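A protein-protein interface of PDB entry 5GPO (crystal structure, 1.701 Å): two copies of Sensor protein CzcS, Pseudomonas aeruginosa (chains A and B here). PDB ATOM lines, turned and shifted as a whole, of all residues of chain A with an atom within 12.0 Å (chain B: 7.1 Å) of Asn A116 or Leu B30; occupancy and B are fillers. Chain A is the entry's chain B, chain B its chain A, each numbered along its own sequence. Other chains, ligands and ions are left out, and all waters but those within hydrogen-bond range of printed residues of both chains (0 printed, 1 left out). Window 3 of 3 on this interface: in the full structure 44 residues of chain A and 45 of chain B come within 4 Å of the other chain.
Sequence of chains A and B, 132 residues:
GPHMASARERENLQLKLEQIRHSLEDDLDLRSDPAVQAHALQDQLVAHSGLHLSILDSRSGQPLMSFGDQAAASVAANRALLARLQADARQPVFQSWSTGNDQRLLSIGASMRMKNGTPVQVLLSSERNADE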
ATOM      1  N   ILE A  55      10.762 -23.890 -11.110  1.00  0.00           N
ATOM      2  CA  ILE A  55       9.317 -23.792 -11.212  1.00  0.00           C
ATOM      3  C   ILE A  55       8.983 -22.375 -11.634  1.00  0.00           C
ATOM      4  O   ILE A  55       9.364 -21.422 -10.948  1.00  0.00           O
ATOM      5  CB  ILE A  55       8.650 -24.168  -9.886  1.00  0.00           C
ATOM      6  CG1 ILE A  55       8.954 -25.648  -9.630  1.00  0.00           C
ATOM      7  CG2 ILE A  55       7.146 -23.881  -9.930  1.00  0.00           C
ATOM      8  CD1 ILE A  55       8.123 -26.259  -8.599  1.00  0.00           C
ATOM      9  N   LEU A  56       8.318 -22.237 -12.787  1.00  0.00           N
ATOM     10  CA  LEU A  56       7.987 -20.951 -13.392  1.00  0.00           C
ATOM     11  C   LEU A  56       6.479 -20.780 -13.423  1.00  0.00           C
ATOM     12  O   LEU A  56       5.752 -21.736 -13.705  1.00  0.00           O
ATOM     13  CB  LEU A  56       8.500 -20.853 -14.836  1.00  0.00           C
ATOM     14  CG  LEU A  56       9.886 -21.415 -15.132  1.00  0.00           C
ATOM     15  CD1 LEU A  56      10.212 -21.260 -16.603  1.00  0.00           C
ATOM     16  CD2 LEU A  56      10.893 -20.707 -14.278  1.00  0.00           C
ATOM     17  N   ASP A  57       6.018 -19.560 -13.135  1.00  0.00           N
ATOM     18  CA  ASP A  57       4.639 -19.174 -13.430  1.00  0.00           C
ATOM     19  C   ASP A  57       4.372 -19.277 -14.933  1.00  0.00           C
ATOM     20  O   ASP A  57       5.020 -18.598 -15.741  1.00  0.00           O
ATOM     21  CB  ASP A  57       4.402 -17.744 -12.921  1.00  0.00           C
ATOM     22  CG  ASP A  57       2.918 -17.394 -12.759  1.00  0.00           C
ATOM     23  OD1 ASP A  57       2.146 -17.549 -13.716  1.00  0.00           O
ATOM     24  OD2 ASP A  57       2.527 -16.944 -11.665  1.00  0.00           O
ATOM     25  N   SER A  58       3.420 -20.145 -15.309  1.00  0.00           N
ATOM     26  CA  SER A  58       3.078 -20.344 -16.713  1.00  0.00           C
ATOM     27  C   SER A  58       2.583 -19.063 -17.373  1.00  0.00           C
ATOM     28  O   SER A  58       2.718 -18.905 -18.585  1.00  0.00           O
ATOM     29  CB  SER A  58       1.987 -21.408 -16.858  1.00  0.00           C
ATOM     30  OG  SER A  58       2.425 -22.691 -16.427  1.00  0.00           O
ATOM     31  N   ARG A  59       1.963 -18.173 -16.610  1.00  0.00           N
ATOM     32  CA  ARG A  59       1.327 -17.016 -17.239  1.00  0.00           C
ATOM     33  C   ARG A  59       2.340 -15.950 -17.615  1.00  0.00           C
ATOM     34  O   ARG A  59       2.204 -15.303 -18.662  1.00  0.00           O
ATOM     35  CB  ARG A  59       0.254 -16.465 -16.307  1.00  0.00           C
ATOM     36  CG  ARG A  59      -0.784 -17.513 -15.963  1.00  0.00           C
ATOM     37  CD  ARG A  59      -1.549 -17.135 -14.720  1.00  0.00           C
ATOM     38  NE  ARG A  59      -0.694 -17.049 -13.543  1.00  0.00           N
ATOM     39  CZ  ARG A  59      -1.139 -16.748 -12.328  1.00  0.00           C
ATOM     40  NH1 ARG A  59      -2.432 -16.507 -12.146  1.00  0.00           N
ATOM     41  NH2 ARG A  59      -0.308 -16.687 -11.300  1.00  0.00           N
ATOM     42  N   LEU A  64       9.178 -18.926 -10.066  1.00  0.00           N
ATOM     43  CA  LEU A  64       8.564 -18.901  -8.750  1.00  0.00           C
ATOM     44  C   LEU A  64       9.453 -19.564  -7.710  1.00  0.00           C
ATOM     45  O   LEU A  64       9.554 -19.068  -6.587  1.00  0.00           O
ATOM     46  CB  LEU A  64       7.184 -19.574  -8.775  1.00  0.00           C
ATOM     47  CG  LEU A  64       6.536 -19.932  -7.426  1.00  0.00           C
ATOM     48  CD1 LEU A  64       6.313 -18.700  -6.551  1.00  0.00           C
ATOM     49  CD2 LEU A  64       5.232 -20.696  -7.598  1.00  0.00           C
ATOM     50  N   MET A  65      10.103 -20.670  -8.070  1.00  0.00           N
ATOM     51  CA  MET A  65      11.043 -21.345  -7.181  1.00  0.00           C
ATOM     52  C   MET A  65      12.216 -21.848  -7.996  1.00  0.00           C
ATOM     53  O   MET A  65      12.040 -22.310  -9.123  1.00  0.00           O
ATOM     54  CB  MET A  65      10.434 -22.546  -6.465  1.00  0.00           C
ATOM     55  CG  MET A  65       9.185 -22.318  -5.679  1.00  0.00           C
ATOM     56  SD  MET A  65       8.688 -23.973  -5.165  1.00  0.00           S
ATOM     57  CE  MET A  65       7.042 -23.647  -4.559  1.00  0.00           C
ATOM     58  N   MET A 112       1.945 -28.026 -14.584  1.00  0.00           N
ATOM     59  CA  MET A 112       1.198 -28.421 -13.396  1.00  0.00           C
ATOM     60  C   MET A 112       0.304 -27.268 -12.982  1.00  0.00           C
ATOM     61  O   MET A 112       0.427 -26.149 -13.485  1.00  0.00           O
ATOM     62  CB  MET A 112       2.126 -28.813 -12.238  1.00  0.00           C
ATOM     63  CG  MET A 112       2.982 -29.989 -12.587  1.00  0.00           C
ATOM     64  SD  MET A 112       3.975 -30.598 -11.234  1.00  0.00           S
ATOM     65  CE  MET A 112       4.968 -31.775 -12.165  1.00  0.00           C
ATOM     66  N   ARG A 113      -0.613 -27.553 -12.063  1.00  0.00           N
ATOM     67  CA  ARG A 113      -1.374 -26.505 -11.398  1.00  0.00           C
ATOM     68  C   ARG A 113      -1.191 -26.679  -9.903  1.00  0.00           C
ATOM     69  O   ARG A 113      -1.594 -27.705  -9.342  1.00  0.00           O
ATOM     70  CB  ARG A 113      -2.857 -26.538 -11.764  1.00  0.00           C
ATOM     71  CG  ARG A 113      -3.632 -25.374 -11.142  1.00  0.00           C
ATOM     72  CD  ARG A 113      -4.989 -25.213 -11.798  1.00  0.00           C
ATOM     73  NE  ARG A 113      -4.870 -25.051 -13.246  1.00  0.00           N
ATOM     74  CZ  ARG A 113      -4.735 -23.883 -13.869  1.00  0.00           C
ATOM     75  NH1 ARG A 113      -4.707 -22.753 -13.177  1.00  0.00           N
ATOM     76  NH2 ARG A 113      -4.630 -23.847 -15.191  1.00  0.00           N
ATOM     77  N   MET A 114      -0.575 -25.686  -9.274  1.00  0.00           N
ATOM     78  CA  MET A 114      -0.384 -25.699  -7.838  1.00  0.00           C
ATOM     79  C   MET A 114      -1.734 -25.657  -7.133  1.00  0.00           C
ATOM     80  O   MET A 114      -2.750 -25.242  -7.699  1.00  0.00           O
ATOM     81  CB  MET A 114       0.492 -24.524  -7.416  1.00  0.00           C
ATOM     82  CG  MET A 114       1.890 -24.587  -8.005  1.00  0.00           C
ATOM     83  SD  MET A 114       2.973 -23.344  -7.314  1.00  0.00           S
ATOM     84  CE  MET A 114       2.814 -23.686  -5.555  1.00  0.00           C
ATOM     85  N   LYS A 115      -1.738 -26.113  -5.877  1.00  0.00           N
ATOM     86  CA  LYS A 115      -2.999 -26.243  -5.157  1.00  0.00           C
ATOM     87  C   LYS A 115      -3.692 -24.897  -5.001  1.00  0.00           C
ATOM     88  O   LYS A 115      -4.926 -24.831  -5.023  1.00  0.00           O
ATOM     89  CB  LYS A 115      -2.768 -26.889  -3.789  1.00  0.00           C
ATOM     90  CG  LYS A 115      -4.056 -27.396  -3.145  1.00  0.00           C
ATOM     91  CD  LYS A 115      -3.882 -27.656  -1.660  1.00  0.00           C
ATOM     92  CE  LYS A 115      -3.092 -28.923  -1.390  1.00  0.00           C
ATOM     93  NZ  LYS A 115      -2.825 -29.092   0.077  1.00  0.00           N
ATOM     94  N   ASN A 116      -2.926 -23.817  -4.876  1.00  0.00           N
ATOM     95  CA  ASN A 116      -3.492 -22.484  -4.743  1.00  0.00           C
ATOM     96  C   ASN A 116      -3.968 -21.899  -6.071  1.00  0.00           C
ATOM     97  O   ASN A 116      -4.375 -20.737  -6.101  1.00  0.00           O
ATOM     98  CB  ASN A 116      -2.476 -21.542  -4.084  1.00  0.00           C
ATOM     99  CG  ASN A 116      -1.140 -21.499  -4.817  1.00  0.00           C
ATOM    100  OD1 ASN A 116      -1.062 -21.746  -6.025  1.00  0.00           O
ATOM    101  ND2 ASN A 116      -0.080 -21.172  -4.084  1.00  0.00           N
ATOM    102  N   GLY A 117      -3.927 -22.669  -7.160  1.00  0.00           N
ATOM    103  CA  GLY A 117      -4.433 -22.244  -8.444  1.00  0.00           C
ATOM    104  C   GLY A 117      -3.372 -21.818  -9.447  1.00  0.00           C
ATOM    105  O   GLY A 117      -3.688 -21.690 -10.635  1.00  0.00           O
ATOM    106  N   THR A 118      -2.136 -21.596  -9.015  1.00  0.00           N
ATOM    107  CA  THR A 118      -1.129 -21.046  -9.941  1.00  0.00           C
ATOM    108  C   THR A 118      -0.756 -22.073 -10.998  1.00  0.00           C
ATOM    109  O   THR A 118      -0.314 -23.175 -10.643  1.00  0.00           O
ATOM    110  CB  THR A 118       0.138 -20.609  -9.204  1.00  0.00           C
ATOM    111  OG1 THR A 118      -0.187 -19.704  -8.144  1.00  0.00           O
ATOM    112  CG2 THR A 118       1.105 -19.913 -10.186  1.00  0.00           C
ATOM    113  N   PRO A 119      -0.878 -21.763 -12.293  1.00  0.00           N
ATOM    114  CA  PRO A 119      -0.367 -22.682 -13.316  1.00  0.00           C
ATOM    115  C   PRO A 119       1.140 -22.505 -13.446  1.00  0.00           C
ATOM    116  O   PRO A 119       1.637 -21.378 -13.564  1.00  0.00           O
ATOM    117  CB  PRO A 119      -1.107 -22.251 -14.589  1.00  0.00           C
ATOM    118  CG  PRO A 119      -1.376 -20.810 -14.373  1.00  0.00           C
ATOM    119  CD  PRO A 119      -1.569 -20.607 -12.892  1.00  0.00           C
ATOM    120  N   VAL A 120       1.870 -23.619 -13.385  1.00  0.00           N
ATOM    121  CA  VAL A 120       3.326 -23.576 -13.355  1.00  0.00           C
ATOM    122  C   VAL A 120       3.904 -24.539 -14.380  1.00  0.00           C
ATOM    123  O   VAL A 120       3.278 -25.538 -14.764  1.00  0.00           O
ATOM    124  CB  VAL A 120       3.913 -23.877 -11.948  1.00  0.00           C
ATOM    125  CG1 VAL A 120       3.512 -22.787 -10.936  1.00  0.00           C
ATOM    126  CG2 VAL A 120       3.550 -25.309 -11.451  1.00  0.00           C
ATOM    127  N   GLN A 121       5.110 -24.220 -14.836  1.00  0.00           N
ATOM    128  CA  GLN A 121       5.930 -25.123 -15.630  1.00  0.00           C
ATOM    129  C   GLN A 121       7.083 -25.584 -14.752  1.00  0.00           C
ATOM    130  O   GLN A 121       7.736 -24.759 -14.104  1.00  0.00           O
ATOM    131  CB  GLN A 121       6.477 -24.449 -16.891  1.00  0.00           C
ATOM    132  CG  GLN A 121       5.440 -23.761 -17.783  1.00  0.00           C
ATOM    133  CD  GLN A 121       4.699 -24.724 -18.694  1.00  0.00           C
ATOM    134  OE1 GLN A 121       4.647 -25.923 -18.441  1.00  0.00           O
ATOM    135  NE2 GLN A 121       4.126 -24.194 -19.771  1.00  0.00           N
ATOM    136  N   VAL A 122       7.328 -26.893 -14.734  1.00  0.00           N
ATOM    137  CA  VAL A 122       8.260 -27.523 -13.802  1.00  0.00           C
ATOM    138  C   VAL A 122       9.393 -28.110 -14.620  1.00  0.00           C
ATOM    139  O   VAL A 122       9.159 -28.945 -15.503  1.00  0.00           O
ATOM    140  CB  VAL A 122       7.581 -28.614 -12.960  1.00  0.00           C
ATOM    141  CG1 VAL A 122       8.631 -29.331 -12.062  1.00  0.00           C
ATOM    142  CG2 VAL A 122       6.449 -28.013 -12.114  1.00  0.00           C
ATOM    143  N   LEU B  24       3.499 -30.509  -5.012  1.00  0.00           N
ATOM    144  CA  LEU B  24       2.968 -29.220  -5.460  1.00  0.00           C
ATOM    145  C   LEU B  24       1.446 -29.194  -5.436  1.00  0.00           C
ATOM    146  O   LEU B  24       0.840 -28.198  -5.029  1.00  0.00           O
ATOM    147  CB  LEU B  24       3.448 -28.911  -6.878  1.00  0.00           C
ATOM    148  CG  LEU B  24       4.752 -28.148  -7.042  1.00  0.00           C
ATOM    149  CD1 LEU B  24       5.138 -28.111  -8.514  1.00  0.00           C
ATOM    150  CD2 LEU B  24       4.607 -26.759  -6.471  1.00  0.00           C
ATOM    151  N   GLU B  25       0.812 -30.262  -5.895  1.00  0.00           N
ATOM    152  CA  GLU B  25      -0.618 -30.226  -6.128  1.00  0.00           C
ATOM    153  C   GLU B  25      -1.439 -30.777  -4.977  1.00  0.00           C
ATOM    154  O   GLU B  25      -2.591 -30.363  -4.806  1.00  0.00           O
ATOM    155  CB  GLU B  25      -0.949 -30.993  -7.412  1.00  0.00           C
ATOM    156  CG  GLU B  25      -0.185 -30.466  -8.634  1.00  0.00           C
ATOM    157  CD  GLU B  25      -0.664 -31.086  -9.924  1.00  0.00           C
ATOM    158  OE1 GLU B  25      -1.282 -32.163  -9.849  1.00  0.00           O
ATOM    159  OE2 GLU B  25      -0.428 -30.500 -11.008  1.00  0.00           O
ATOM    160  N   ASP B  27       0.033 -31.787  -1.446  1.00  0.00           N
ATOM    161  CA  ASP B  27       0.510 -31.579  -0.089  1.00  0.00           C
ATOM    162  C   ASP B  27       0.757 -30.118   0.247  1.00  0.00           C
ATOM    163  O   ASP B  27       0.878 -29.785   1.433  1.00  0.00           O
ATOM    164  CB  ASP B  27       1.792 -32.385   0.134  1.00  0.00           C
ATOM    165  CG  ASP B  27       1.514 -33.854   0.387  1.00  0.00           C
ATOM    166  OD1 ASP B  27       0.324 -34.261   0.367  1.00  0.00           O
ATOM    167  OD2 ASP B  27       2.489 -34.592   0.599  1.00  0.00           O
ATOM    168  N   LEU B  28       0.832 -29.258  -0.770  1.00  0.00           N
ATOM    169  CA  LEU B  28       1.081 -27.835  -0.606  1.00  0.00           C
ATOM    170  C   LEU B  28       0.202 -27.256   0.482  1.00  0.00           C
ATOM    171  O   LEU B  28      -1.026 -27.359   0.424  1.00  0.00           O
ATOM    172  CB  LEU B  28       0.814 -27.109  -1.928  1.00  0.00           C
ATOM    173  CG  LEU B  28       1.068 -25.598  -1.929  1.00  0.00           C
ATOM    174  CD1 LEU B  28       2.559 -25.343  -2.171  1.00  0.00           C
ATOM    175  CD2 LEU B  28       0.227 -24.904  -2.987  1.00  0.00           C
ATOM    176  N   ASP B  29       0.839 -26.637   1.458  1.00  0.00           N
ATOM    177  CA  ASP B  29       0.126 -25.972   2.538  1.00  0.00           C
ATOM    178  C   ASP B  29      -0.308 -24.588   2.072  1.00  0.00           C
ATOM    179  O   ASP B  29       0.524 -23.689   1.920  1.00  0.00           O
ATOM    180  CB  ASP B  29       1.022 -25.881   3.767  1.00  0.00           C
ATOM    181  CG  ASP B  29       0.250 -25.574   5.022  1.00  0.00           C
ATOM    182  OD1 ASP B  29      -0.799 -24.898   4.925  1.00  0.00           O
ATOM    183  OD2 ASP B  29       0.707 -26.003   6.103  1.00  0.00           O
ATOM    184  N   LEU B  30      -1.613 -24.407   1.867  1.00  0.00           N
ATOM    185  CA  LEU B  30      -2.114 -23.104   1.443  1.00  0.00           C
ATOM    186  C   LEU B  30      -1.852 -22.022   2.483  1.00  0.00           C
ATOM    187  O   LEU B  30      -1.797 -20.839   2.130  1.00  0.00           O
ATOM    188  CB  LEU B  30      -3.609 -23.187   1.143  1.00  0.00           C
ATOM    189  CG  LEU B  30      -3.992 -24.064  -0.046  1.00  0.00           C
ATOM    190  CD1 LEU B  30      -5.496 -24.045  -0.272  1.00  0.00           C
ATOM    191  CD2 LEU B  30      -3.252 -23.599  -1.292  1.00  0.00           C
ATOM    192  N   ARG B  31      -1.676 -22.400   3.752  1.00  0.00           N
ATOM    193  CA  ARG B  31      -1.451 -21.427   4.814  1.00  0.00           C
ATOM    194  C   ARG B  31      -0.022 -20.904   4.844  1.00  0.00           C
ATOM    195  O   ARG B  31       0.232 -19.875   5.481  1.00  0.00           O
ATOM    196  CB  ARG B  31      -1.801 -22.044   6.173  1.00  0.00           C
ATOM    197  N   SER B  32       0.911 -21.578   4.180  1.00  0.00           N
ATOM    198  CA  SER B  32       2.308 -21.175   4.219  1.00  0.00           C
ATOM    199  C   SER B  32       2.579 -20.067   3.210  1.00  0.00           C
ATOM    200  O   SER B  32       1.917 -19.965   2.175  1.00  0.00           O
ATOM    201  CB  SER B  32       3.224 -22.365   3.922  1.00  0.00           C
ATOM    202  OG  SER B  32       2.949 -23.477   4.758  1.00  0.00           O
ATOM    203  N   ASP B  33       3.571 -19.236   3.525  1.00  0.00           N
ATOM    204  CA  ASP B  33       4.066 -18.233   2.592  1.00  0.00           C
ATOM    205  C   ASP B  33       4.975 -18.892   1.559  1.00  0.00           C
ATOM    206  O   ASP B  33       5.410 -20.033   1.740  1.00  0.00           O
ATOM    207  CB  ASP B  33       4.781 -17.115   3.359  1.00  0.00           C
ATOM    208  CG  ASP B  33       5.956 -17.611   4.193  1.00  0.00           C
ATOM    209  OD1 ASP B  33       6.658 -18.557   3.774  1.00  0.00           O
ATOM    210  OD2 ASP B  33       6.188 -17.034   5.279  1.00  0.00           O
ATOM    211  N   GLN B  37       6.735 -22.678   1.470  1.00  0.00           N
ATOM    212  CA  GLN B  37       6.352 -23.631   0.434  1.00  0.00           C
ATOM    213  C   GLN B  37       7.565 -24.053  -0.389  1.00  0.00           C
ATOM    214  O   GLN B  37       7.733 -25.235  -0.701  1.00  0.00           O
ATOM    215  CB  GLN B  37       5.255 -23.038  -0.465  1.00  0.00           C
ATOM    216  CG  GLN B  37       3.928 -22.778   0.264  1.00  0.00           C
ATOM    217  CD  GLN B  37       2.826 -22.202  -0.623  1.00  0.00           C
ATOM    218  OE1 GLN B  37       3.086 -21.655  -1.692  1.00  0.00           O
ATOM    219  NE2 GLN B  37       1.582 -22.324  -0.170  1.00  0.00           N
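Leu A56 touches none of the printed residues of chain B. Of the printed residues of chain B, Met A114 touches Leu B24 and Leu B28. Gly A117 touches none of the printed residues of chain B. Printed residues of chain B within 4 Å of Val A122: Leu B24 (3.8 Å). Of the printed residues of chain A, Leu B24 touches Ile A55 (3.5 Å), Met A112 (3.9 Å), Met A114 (3.7 Å), Lys A115 (3.4 Å) and Val A122 (3.8 Å). Of chain A, only Met A114 (3.8 Å), Lys A115 (2.5 Å) and Asn A116 (3.8 Å) come within 4 Å of Leu B28. No residue of chain A comes within 4 Å of Asp B29. No residue of chain A comes within 4 Å of Arg B31. No residue of chain A comes within 4 Å of Ser B32. Of the printed residues of chain A, Gln B37 touches Asn A116. The nearest printed residue of chain B that does not touch Asn A116 is Leu B24 (5.8 Å). The nearest residue of chain A that does not touch Leu B30 is Gly A117 (6.0 Å).
The backbone carbonyl oxygen (O) of Leu B24 lies within hydrogen-bond range of the backbone NH (N) of Lys A115. OE2 of Glu B25 sits at hydrogen-bond distance from N of Arg A113. O of Leu B28 is in hydrogen-bond range of NZ of Lys A115, 2.5 Å away.
Ile A55 touches Leu B24 (CD1 to CD1, 3.5 Å). Leu B24 touches Met A112. Glu B25 touches Met A112 (OE2 to CB, 3.3 Å). Met A114 touches Leu B24. Leu B28 touches Met A114. O of Glu B25 touches CB of Lys A115, at 3.6 Å. CD of Lys A115 touches CG of Leu B30, 3.9 Å away. Asn A116 touches Leu B28 (N to CD2, 3.8 Å). Asn A116 touches Gln B37 (ND2 to OE1, 3.997 Å). CG2 of Val A122 touches CD1 of Leu B24 (3.8 Å).
NE2 of Gln B37 sits at hydrogen-bond distance from O of Asp B29 (2.7 Å). O of Ser B32 lies within hydrogen-bond range of NE2 of Gln B37. O of Ile A55 lies within hydrogen-bond range of N of Leu A64, 2.7 Å away. The backbone carbonyl oxygen (O) of Met A65 sits at hydrogen-bond distance from the backbone NH (N) of Ile A55. NH1 of Arg A113 lies within hydrogen-bond range of O of Gly A117 (2.9 Å). The side-chain hydroxyl of Thr A118 sits at hydrogen-bond distance from the side-chain amide oxygen of Asn A116 (3.1 Å).
No position is printed for both chains.
Of the 10 printed residues of chain B, 6 touch a printed residue of chain A. Hydrophobic or aromatic side chains of chain B within 4 Å of the printed part of chain A: Leu B24, Leu B28 and Leu B30. Printed residues of chain A that touch a printed residue of chain B: Ile A55, Met A112, Arg A113, Met A114, Lys A115, Asn A116 and Val A122. Hydrophobic or aromatic side chains of chain A within 4 Å of the printed part of chain B: Ile A55, Met A112, Met A114 and Val A122. Among the printed residues, 15 pairs touch across the chains.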
